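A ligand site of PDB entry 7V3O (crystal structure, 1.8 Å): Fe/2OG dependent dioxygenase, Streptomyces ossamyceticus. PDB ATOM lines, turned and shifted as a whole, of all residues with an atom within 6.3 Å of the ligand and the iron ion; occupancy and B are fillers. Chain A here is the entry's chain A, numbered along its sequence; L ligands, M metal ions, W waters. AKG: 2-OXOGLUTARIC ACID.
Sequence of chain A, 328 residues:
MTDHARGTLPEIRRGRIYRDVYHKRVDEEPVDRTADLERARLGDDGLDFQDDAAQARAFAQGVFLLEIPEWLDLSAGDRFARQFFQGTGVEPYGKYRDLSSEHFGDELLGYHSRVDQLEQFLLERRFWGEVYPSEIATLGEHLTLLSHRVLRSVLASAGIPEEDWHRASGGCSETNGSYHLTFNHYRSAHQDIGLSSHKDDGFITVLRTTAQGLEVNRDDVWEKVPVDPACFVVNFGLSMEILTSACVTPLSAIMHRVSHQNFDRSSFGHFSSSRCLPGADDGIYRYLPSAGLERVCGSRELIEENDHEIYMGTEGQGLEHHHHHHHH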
ATOM      1  N   LEU A 118     -22.257  11.048 -19.061  1.00  0.00           N
ATOM      2  CA  LEU A 118     -21.021  11.830 -19.090  1.00  0.00           C
ATOM      3  C   LEU A 118     -20.074  11.454 -20.237  1.00  0.00           C
ATOM      4  O   LEU A 118     -19.853  10.274 -20.516  1.00  0.00           O
ATOM      5  CB  LEU A 118     -20.292  11.591 -17.771  1.00  0.00           C
ATOM      6  CG  LEU A 118     -18.918  12.224 -17.602  1.00  0.00           C
ATOM      7  CD1 LEU A 118     -19.149  13.733 -17.538  1.00  0.00           C
ATOM      8  CD2 LEU A 118     -18.306  11.714 -16.309  1.00  0.00           C
ATOM      9  N   GLN A 120     -15.947  13.083 -21.199  1.00  0.00           N
ATOM     10  CA  GLN A 120     -14.949  13.912 -20.518  1.00  0.00           C
ATOM     11  C   GLN A 120     -13.752  14.188 -21.405  1.00  0.00           C
ATOM     12  O   GLN A 120     -13.417  13.412 -22.305  1.00  0.00           O
ATOM     13  CB  GLN A 120     -14.439  13.230 -19.251  1.00  0.00           C
ATOM     14  CG  GLN A 120     -15.458  13.002 -18.166  1.00  0.00           C
ATOM     15  CD  GLN A 120     -14.815  12.378 -16.932  1.00  0.00           C
ATOM     16  OE1 GLN A 120     -14.391  11.226 -16.969  1.00  0.00           O
ATOM     17  NE2 GLN A 120     -14.730  13.142 -15.827  1.00  0.00           N
ATOM     18  N   THR A 182     -10.211  18.678 -15.706  1.00  0.00           N
ATOM     19  CA  THR A 182     -11.088  17.700 -16.345  1.00  0.00           C
ATOM     20  C   THR A 182     -12.387  18.392 -16.722  1.00  0.00           C
ATOM     21  O   THR A 182     -12.983  19.056 -15.873  1.00  0.00           O
ATOM     22  CB  THR A 182     -11.363  16.550 -15.372  1.00  0.00           C
ATOM     23  OG1 THR A 182     -10.172  15.794 -15.187  1.00  0.00           O
ATOM     24  CG2 THR A 182     -12.447  15.604 -15.943  1.00  0.00           C
ATOM     25  N   ASN A 184     -16.302  18.174 -18.337  1.00  0.00           N
ATOM     26  CA  ASN A 184     -17.421  17.228 -18.306  1.00  0.00           C
ATOM     27  C   ASN A 184     -18.579  17.732 -19.161  1.00  0.00           C
ATOM     28  O   ASN A 184     -18.999  18.889 -19.025  1.00  0.00           O
ATOM     29  CB  ASN A 184     -17.960  17.037 -16.895  1.00  0.00           C
ATOM     30  CG  ASN A 184     -16.955  16.419 -15.951  1.00  0.00           C
ATOM     31  OD1 ASN A 184     -16.116  15.616 -16.343  1.00  0.00           O
ATOM     32  ND2 ASN A 184     -17.082  16.747 -14.671  1.00  0.00           N
ATOM     33  N   TYR A 186     -22.601  16.290 -20.204  1.00  0.00           N
ATOM     34  CA  TYR A 186     -23.637  15.286 -19.963  1.00  0.00           C
ATOM     35  C   TYR A 186     -24.547  15.233 -21.182  1.00  0.00           C
ATOM     36  O   TYR A 186     -25.128  16.242 -21.561  1.00  0.00           O
ATOM     37  CB  TYR A 186     -24.421  15.613 -18.684  1.00  0.00           C
ATOM     38  CG  TYR A 186     -23.481  15.534 -17.497  1.00  0.00           C
ATOM     39  CD1 TYR A 186     -22.673  16.616 -17.141  1.00  0.00           C
ATOM     40  CD2 TYR A 186     -23.326  14.338 -16.805  1.00  0.00           C
ATOM     41  CE1 TYR A 186     -21.752  16.510 -16.090  1.00  0.00           C
ATOM     42  CE2 TYR A 186     -22.401  14.235 -15.730  1.00  0.00           C
ATOM     43  CZ  TYR A 186     -21.627  15.334 -15.390  1.00  0.00           C
ATOM     44  OH  TYR A 186     -20.721  15.210 -14.339  1.00  0.00           O
ATOM     45  N   LEU A 195     -23.977  10.745 -13.946  1.00  0.00           N
ATOM     46  CA  LEU A 195     -22.737  10.130 -13.522  1.00  0.00           C
ATOM     47  C   LEU A 195     -23.056   9.380 -12.245  1.00  0.00           C
ATOM     48  O   LEU A 195     -23.585   9.969 -11.291  1.00  0.00           O
ATOM     49  CB  LEU A 195     -21.631  11.176 -13.287  1.00  0.00           C
ATOM     50  CG  LEU A 195     -20.348  10.688 -12.614  1.00  0.00           C
ATOM     51  CD1 LEU A 195     -19.664   9.612 -13.469  1.00  0.00           C
ATOM     52  CD2 LEU A 195     -19.394  11.906 -12.339  1.00  0.00           C
ATOM     53  N   HIS A 198     -20.136   7.851  -6.778  1.00  0.00           N
ATOM     54  CA  HIS A 198     -18.725   7.566  -6.627  1.00  0.00           C
ATOM     55  C   HIS A 198     -18.146   8.488  -5.561  1.00  0.00           C
ATOM     56  O   HIS A 198     -18.775   9.457  -5.115  1.00  0.00           O
ATOM     57  CB  HIS A 198     -17.970   7.747  -7.946  1.00  0.00           C
ATOM     58  CG  HIS A 198     -17.927   9.163  -8.396  1.00  0.00           C
ATOM     59  ND1 HIS A 198     -19.028   9.824  -8.882  1.00  0.00           N
ATOM     60  CD2 HIS A 198     -16.918  10.080  -8.376  1.00  0.00           C
ATOM     61  CE1 HIS A 198     -18.724  11.078  -9.125  1.00  0.00           C
ATOM     62  NE2 HIS A 198     -17.449  11.254  -8.844  1.00  0.00           N
ATOM     63  N   LYS A 199     -16.930   8.161  -5.164  1.00  0.00           N
ATOM     64  CA  LYS A 199     -16.049   9.022  -4.392  1.00  0.00           C
ATOM     65  C   LYS A 199     -14.865   9.374  -5.277  1.00  0.00           C
ATOM     66  O   LYS A 199     -14.417   8.542  -6.069  1.00  0.00           O
ATOM     67  CB  LYS A 199     -15.593   8.307  -3.116  1.00  0.00           C
ATOM     68  CG  LYS A 199     -16.778   7.816  -2.274  1.00  0.00           C
ATOM     69  CD  LYS A 199     -16.369   7.114  -0.975  1.00  0.00           C
ATOM     70  CE  LYS A 199     -17.582   6.410  -0.363  1.00  0.00           C
ATOM     71  NZ  LYS A 199     -17.722   6.578   1.108  1.00  0.00           N
ATOM     72  N   ASP A 200     -14.376  10.616  -5.184  1.00  0.00           N
ATOM     73  CA  ASP A 200     -13.226  11.020  -5.985  1.00  0.00           C
ATOM     74  C   ASP A 200     -11.975  10.345  -5.474  1.00  0.00           C
ATOM     75  O   ASP A 200     -11.848  10.055  -4.276  1.00  0.00           O
ATOM     76  CB  ASP A 200     -13.054  12.544  -5.957  1.00  0.00           C
ATOM     77  CG  ASP A 200     -14.143  13.261  -6.718  1.00  0.00           C
ATOM     78  OD1 ASP A 200     -14.836  12.566  -7.503  1.00  0.00           O
ATOM     79  OD2 ASP A 200     -14.332  14.480  -6.545  1.00  0.00           O
ATOM     80  N   THR A 205     -10.911  18.130  -4.556  1.00  0.00           N
ATOM     81  CA  THR A 205     -11.550  18.450  -5.816  1.00  0.00           C
ATOM     82  C   THR A 205     -12.123  19.837  -5.726  1.00  0.00           C
ATOM     83  O   THR A 205     -12.863  20.149  -4.777  1.00  0.00           O
ATOM     84  CB  THR A 205     -12.690  17.468  -6.131  1.00  0.00           C
ATOM     85  OG1 THR A 205     -12.161  16.150  -6.268  1.00  0.00           O
ATOM     86  CG2 THR A 205     -13.404  17.895  -7.407  1.00  0.00           C
ATOM     87  N   LEU A 207     -14.621  22.030  -7.876  1.00  0.00           N
ATOM     88  CA  LEU A 207     -15.574  21.797  -8.968  1.00  0.00           C
ATOM     89  C   LEU A 207     -16.286  23.084  -9.351  1.00  0.00           C
ATOM     90  O   LEU A 207     -16.850  23.785  -8.504  1.00  0.00           O
ATOM     91  CB  LEU A 207     -16.610  20.744  -8.560  1.00  0.00           C
ATOM     92  CG  LEU A 207     -17.679  20.461  -9.634  1.00  0.00           C
ATOM     93  CD1 LEU A 207     -17.074  19.656 -10.806  1.00  0.00           C
ATOM     94  CD2 LEU A 207     -18.822  19.704  -9.012  1.00  0.00           C
ATOM     95  N   ARG A 208     -16.283  23.384 -10.646  1.00  0.00           N
ATOM     96  CA  ARG A 208     -17.005  24.535 -11.180  1.00  0.00           C
ATOM     97  C   ARG A 208     -18.257  23.996 -11.874  1.00  0.00           C
ATOM     98  O   ARG A 208     -18.183  23.334 -12.918  1.00  0.00           O
ATOM     99  CB  ARG A 208     -16.102  25.359 -12.085  1.00  0.00           C
ATOM    100  CG  ARG A 208     -16.739  26.417 -12.972  1.00  0.00           C
ATOM    101  CD  ARG A 208     -17.855  27.150 -12.373  1.00  0.00           C
ATOM    102  NE  ARG A 208     -18.298  28.315 -13.134  1.00  0.00           N
ATOM    103  CZ  ARG A 208     -18.833  29.354 -12.516  1.00  0.00           C
ATOM    104  NH1 ARG A 208     -18.907  29.306 -11.199  1.00  0.00           N
ATOM    105  NH2 ARG A 208     -19.249  30.434 -13.193  1.00  0.00           N
ATOM    106  N   THR A 209     -19.402  24.245 -11.275  1.00  0.00           N
ATOM    107  CA  THR A 209     -20.675  23.834 -11.830  1.00  0.00           C
ATOM    108  C   THR A 209     -21.625  25.020 -11.770  1.00  0.00           C
ATOM    109  O   THR A 209     -21.561  25.813 -10.819  1.00  0.00           O
ATOM    110  CB  THR A 209     -21.266  22.624 -11.072  1.00  0.00           C
ATOM    111  OG1 THR A 209     -22.495  22.265 -11.691  1.00  0.00           O
ATOM    112  CG2 THR A 209     -21.524  22.951  -9.611  1.00  0.00           C
ATOM    113  N   GLY A 213     -27.931  19.356 -10.783  1.00  0.00           N
ATOM    114  CA  GLY A 213     -27.607  17.990 -11.133  1.00  0.00           C
ATOM    115  C   GLY A 213     -26.761  17.263 -10.118  1.00  0.00           C
ATOM    116  O   GLY A 213     -26.877  16.050  -9.927  1.00  0.00           O
ATOM    117  N   LEU A 214     -25.847  18.001  -9.488  1.00  0.00           N
ATOM    118  CA  LEU A 214     -24.973  17.376  -8.513  1.00  0.00           C
ATOM    119  C   LEU A 214     -25.773  17.038  -7.254  1.00  0.00           C
ATOM    120  O   LEU A 214     -26.581  17.843  -6.784  1.00  0.00           O
ATOM    121  CB  LEU A 214     -23.810  18.312  -8.172  1.00  0.00           C
ATOM    122  CG  LEU A 214     -22.772  17.747  -7.190  1.00  0.00           C
ATOM    123  CD1 LEU A 214     -22.064  16.531  -7.751  1.00  0.00           C
ATOM    124  CD2 LEU A 214     -21.760  18.852  -6.884  1.00  0.00           C
ATOM    125  N   ASN A 235     -14.776  19.274  -2.386  1.00  0.00           N
ATOM    126  CA  ASN A 235     -14.886  18.059  -1.589  1.00  0.00           C
ATOM    127  C   ASN A 235     -13.545  17.342  -1.574  1.00  0.00           C
ATOM    128  O   ASN A 235     -12.596  17.727  -2.265  1.00  0.00           O
ATOM    129  CB  ASN A 235     -15.998  17.123  -2.093  1.00  0.00           C
ATOM    130  CG  ASN A 235     -15.775  16.671  -3.547  1.00  0.00           C
ATOM    131  OD1 ASN A 235     -16.279  17.283  -4.474  1.00  0.00           O
ATOM    132  ND2 ASN A 235     -15.056  15.575  -3.727  1.00  0.00           N
ATOM    133  N   HIS A 256     -21.044  11.025  -4.232  1.00  0.00           N
ATOM    134  CA  HIS A 256     -21.834  11.997  -4.976  1.00  0.00           C
ATOM    135  C   HIS A 256     -22.081  11.478  -6.397  1.00  0.00           C
ATOM    136  O   HIS A 256     -21.454  10.526  -6.857  1.00  0.00           O
ATOM    137  CB  HIS A 256     -21.150  13.380  -5.015  1.00  0.00           C
ATOM    138  CG  HIS A 256     -19.757  13.351  -5.535  1.00  0.00           C
ATOM    139  ND1 HIS A 256     -18.719  12.767  -4.847  1.00  0.00           N
ATOM    140  CD2 HIS A 256     -19.237  13.807  -6.698  1.00  0.00           C
ATOM    141  CE1 HIS A 256     -17.610  12.866  -5.562  1.00  0.00           C
ATOM    142  NE2 HIS A 256     -17.905  13.509  -6.687  1.00  0.00           N
ATOM    143  N   ARG A 257     -23.038  12.101  -7.070  1.00  0.00           N
ATOM    144  CA  ARG A 257     -23.477  11.641  -8.378  1.00  0.00           C
ATOM    145  C   ARG A 257     -24.071  12.828  -9.120  1.00  0.00           C
ATOM    146  O   ARG A 257     -24.302  13.887  -8.526  1.00  0.00           O
ATOM    147  CB  ARG A 257     -24.519  10.500  -8.234  1.00  0.00           C
ATOM    148  CG  ARG A 257     -25.849  10.991  -7.667  1.00  0.00           C
ATOM    149  CD  ARG A 257     -26.837   9.839  -7.394  1.00  0.00           C
ATOM    150  NE  ARG A 257     -28.063  10.323  -6.785  1.00  0.00           N
ATOM    151  CZ  ARG A 257     -28.962   9.552  -6.165  1.00  0.00           C
ATOM    152  NH1 ARG A 257     -28.773   8.245  -6.062  1.00  0.00           N
ATOM    153  NH2 ARG A 257     -30.057  10.109  -5.641  1.00  0.00           N
ATOM    154  N   VAL A 258     -24.372  12.642 -10.402  1.00  0.00           N
ATOM    155  CA  VAL A 258     -25.089  13.648 -11.178  1.00  0.00           C
ATOM    156  C   VAL A 258     -26.344  12.966 -11.707  1.00  0.00           C
ATOM    157  O   VAL A 258     -26.235  11.918 -12.347  1.00  0.00           O
ATOM    158  CB  VAL A 258     -24.253  14.210 -12.331  1.00  0.00           C
ATOM    159  CG1 VAL A 258     -25.089  15.121 -13.223  1.00  0.00           C
ATOM    160  CG2 VAL A 258     -23.004  14.978 -11.782  1.00  0.00           C
ATOM    161  N   ARG A 265     -25.767  19.433 -19.942  1.00  0.00           N
ATOM    162  CA  ARG A 265     -25.156  20.079 -18.792  1.00  0.00           C
ATOM    163  C   ARG A 265     -23.659  19.956 -18.995  1.00  0.00           C
ATOM    164  O   ARG A 265     -23.177  18.984 -19.594  1.00  0.00           O
ATOM    165  CB  ARG A 265     -25.621  19.421 -17.487  1.00  0.00           C
ATOM    166  CG  ARG A 265     -24.978  19.945 -16.159  1.00  0.00           C
ATOM    167  CD  ARG A 265     -25.427  19.077 -14.979  1.00  0.00           C
ATOM    168  NE  ARG A 265     -24.901  19.522 -13.689  1.00  0.00           N
ATOM    169  CZ  ARG A 265     -23.725  19.147 -13.168  1.00  0.00           C
ATOM    170  NH1 ARG A 265     -22.962  18.315 -13.826  1.00  0.00           N
ATOM    171  NH2 ARG A 265     -23.326  19.611 -11.970  1.00  0.00           N
ATOM    172  N   SER A 266     -22.906  20.929 -18.479  1.00  0.00           N
ATOM    173  CA  SER A 266     -21.459  20.795 -18.498  1.00  0.00           C
ATOM    174  C   SER A 266     -20.904  21.381 -17.215  1.00  0.00           C
ATOM    175  O   SER A 266     -21.573  22.140 -16.502  1.00  0.00           O
ATOM    176  CB  SER A 266     -20.828  21.465 -19.732  1.00  0.00           C
ATOM    177  OG  SER A 266     -21.009  22.887 -19.695  1.00  0.00           O
ATOM    178  N   SER A 267     -19.658  20.999 -16.926  1.00  0.00           N
ATOM    179  CA  SER A 267     -18.962  21.420 -15.716  1.00  0.00           C
ATOM    180  C   SER A 267     -17.479  21.148 -15.929  1.00  0.00           C
ATOM    181  O   SER A 267     -17.075  20.515 -16.898  1.00  0.00           O
ATOM    182  CB  SER A 267     -19.472  20.686 -14.470  1.00  0.00           C
ATOM    183  OG  SER A 267     -19.204  19.284 -14.565  1.00  0.00           O
ATOM    184  N   PHE A 268     -16.649  21.629 -14.998  1.00  0.00           N
ATOM    185  CA  PHE A 268     -15.268  21.188 -15.021  1.00  0.00           C
ATOM    186  C   PHE A 268     -14.709  21.234 -13.613  1.00  0.00           C
ATOM    187  O   PHE A 268     -15.257  21.912 -12.732  1.00  0.00           O
ATOM    188  CB  PHE A 268     -14.387  22.012 -15.994  1.00  0.00           C
ATOM    189  CG  PHE A 268     -14.208  23.460 -15.633  1.00  0.00           C
ATOM    190  CD1 PHE A 268     -13.139  23.869 -14.839  1.00  0.00           C
ATOM    191  CD2 PHE A 268     -15.074  24.419 -16.142  1.00  0.00           C
ATOM    192  CE1 PHE A 268     -12.966  25.225 -14.534  1.00  0.00           C
ATOM    193  CE2 PHE A 268     -14.899  25.793 -15.865  1.00  0.00           C
ATOM    194  CZ  PHE A 268     -13.843  26.192 -15.038  1.00  0.00           C
ATOM    195  N   PHE A 271      -8.564  18.429  -9.927  1.00  0.00           N
ATOM    196  CA  PHE A 271      -8.436  17.261  -9.054  1.00  0.00           C
ATOM    197  C   PHE A 271      -6.979  17.105  -8.629  1.00  0.00           C
ATOM    198  O   PHE A 271      -6.106  16.999  -9.486  1.00  0.00           O
ATOM    199  CB  PHE A 271      -8.919  16.000  -9.774  1.00  0.00           C
ATOM    200  CG  PHE A 271     -10.392  16.026 -10.186  1.00  0.00           C
ATOM    201  CD1 PHE A 271     -10.817  16.818 -11.250  1.00  0.00           C
ATOM    202  CD2 PHE A 271     -11.319  15.258  -9.507  1.00  0.00           C
ATOM    203  CE1 PHE A 271     -12.194  16.827 -11.638  1.00  0.00           C
ATOM    204  CE2 PHE A 271     -12.673  15.264  -9.865  1.00  0.00           C
ATOM    205  CZ  PHE A 271     -13.111  16.052 -10.927  1.00  0.00           C
HETATM  206  C1  AKG L   1     -16.413  14.198 -11.259  1.00  0.00           C
HETATM  207  O1  AKG L   1     -15.768  13.385 -10.542  1.00  0.00           O
HETATM  208  O2  AKG L   1     -15.955  14.563 -12.368  1.00  0.00           O
HETATM  209  C2  AKG L   1     -17.714  14.713 -10.837  1.00  0.00           C
HETATM  210  O5  AKG L   1     -18.251  14.333  -9.801  1.00  0.00           O
HETATM  211  C3  AKG L   1     -18.460  15.698 -11.715  1.00  0.00           C
HETATM  212  C4  AKG L   1     -19.602  16.383 -10.963  1.00  0.00           C
HETATM  213  C5  AKG L   1     -20.336  17.378 -11.836  1.00  0.00           C
HETATM  214  O3  AKG L   1     -21.050  18.220 -11.257  1.00  0.00           O
HETATM  215  O4  AKG L   1     -20.220  17.371 -13.091  1.00  0.00           O
HETATM  216 FE    FE M   1     -16.725  13.357  -8.544  1.00  0.00          FE
HETATM  217  O   HOH W   1     -16.009  15.491  -8.192  1.00  0.00           O
HETATM  218  O   HOH W   2     -13.677  13.259 -13.127  1.00  0.00           O
HETATM  219  O   HOH W   3     -13.935  11.379 -10.345  1.00  0.00           O
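The side-chain carboxylate (OD2) of Asp 200 is in hydrogen-bond range of the side-chain amide nitrogen (ND2) of Asn 235, 3.1 Å away.
The side-chain carboxylate (OD2) of Asp 200 sits at hydrogen-bond distance from the side-chain hydroxyl (OG1) of Thr 205 (2.8 Å).
The backbone NH of Tyr 186 lies within hydrogen-bond range of the backbone carbonyl oxygen of Arg 265.
O of Ser 267 lies within hydrogen-bond range of N of Asn 184.
The side-chain hydroxyl (OG1) of Thr 209 sits at hydrogen-bond distance from the guanidinium group (NH2) of Arg 265, at 2.8 Å.
NE2 of Gln 120 sits at hydrogen-bond distance from OD1 of Asn 184 (2.9 Å).
The backbone carbonyl oxygen of Leu 195 is in hydrogen-bond range of the backbone NH of Val 258, 2.9 Å away.
Gln 120 touches the ligand.
Leu 195 touches the ligand.
Leu 207 touches the ligand.
Val 258 touches the ligand.
Phe 271 touches the ligand.
Hydrophobic or aromatic side chains within 4 Å of the ligand: Tyr 186, Leu 195, His 198, Leu 207, His 256, Val 258 and Phe 271.
Within 4 Å of the ligand: Gln 120, Asn 184, Tyr 186, Leu 195, His 198, Asp 200, Leu 207, His 256, Val 258, Arg 265, Ser 267 and Phe 271.
The iron ion is bound by O5 of the ligand, NE2 of His 256, O1 of the ligand, NE2 of His 198, water W1 and OD1 of Asp 200.
The iron ion has six donor atoms within binding distance.
Water W2 bridges an oxygen (O2) of the ligand (2.7 Å) and the side-chain amide nitrogen (NE2) of Gln 120 (2.9 Å).
OH of Tyr 186 sits at hydrogen-bond distance from O4 of the ligand.
The side-chain hydroxyl of Ser 267 sits at hydrogen-bond distance from an oxygen (O4) of the ligand (2.6 Å).
NH2 of Arg 265 is in salt-bridge range of O3 of the ligand, at 2.8 Å.
The side-chain amide nitrogen (ND2) of Asn 184 sits at hydrogen-bond distance from an oxygen (O2) of the ligand (3.4 Å).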
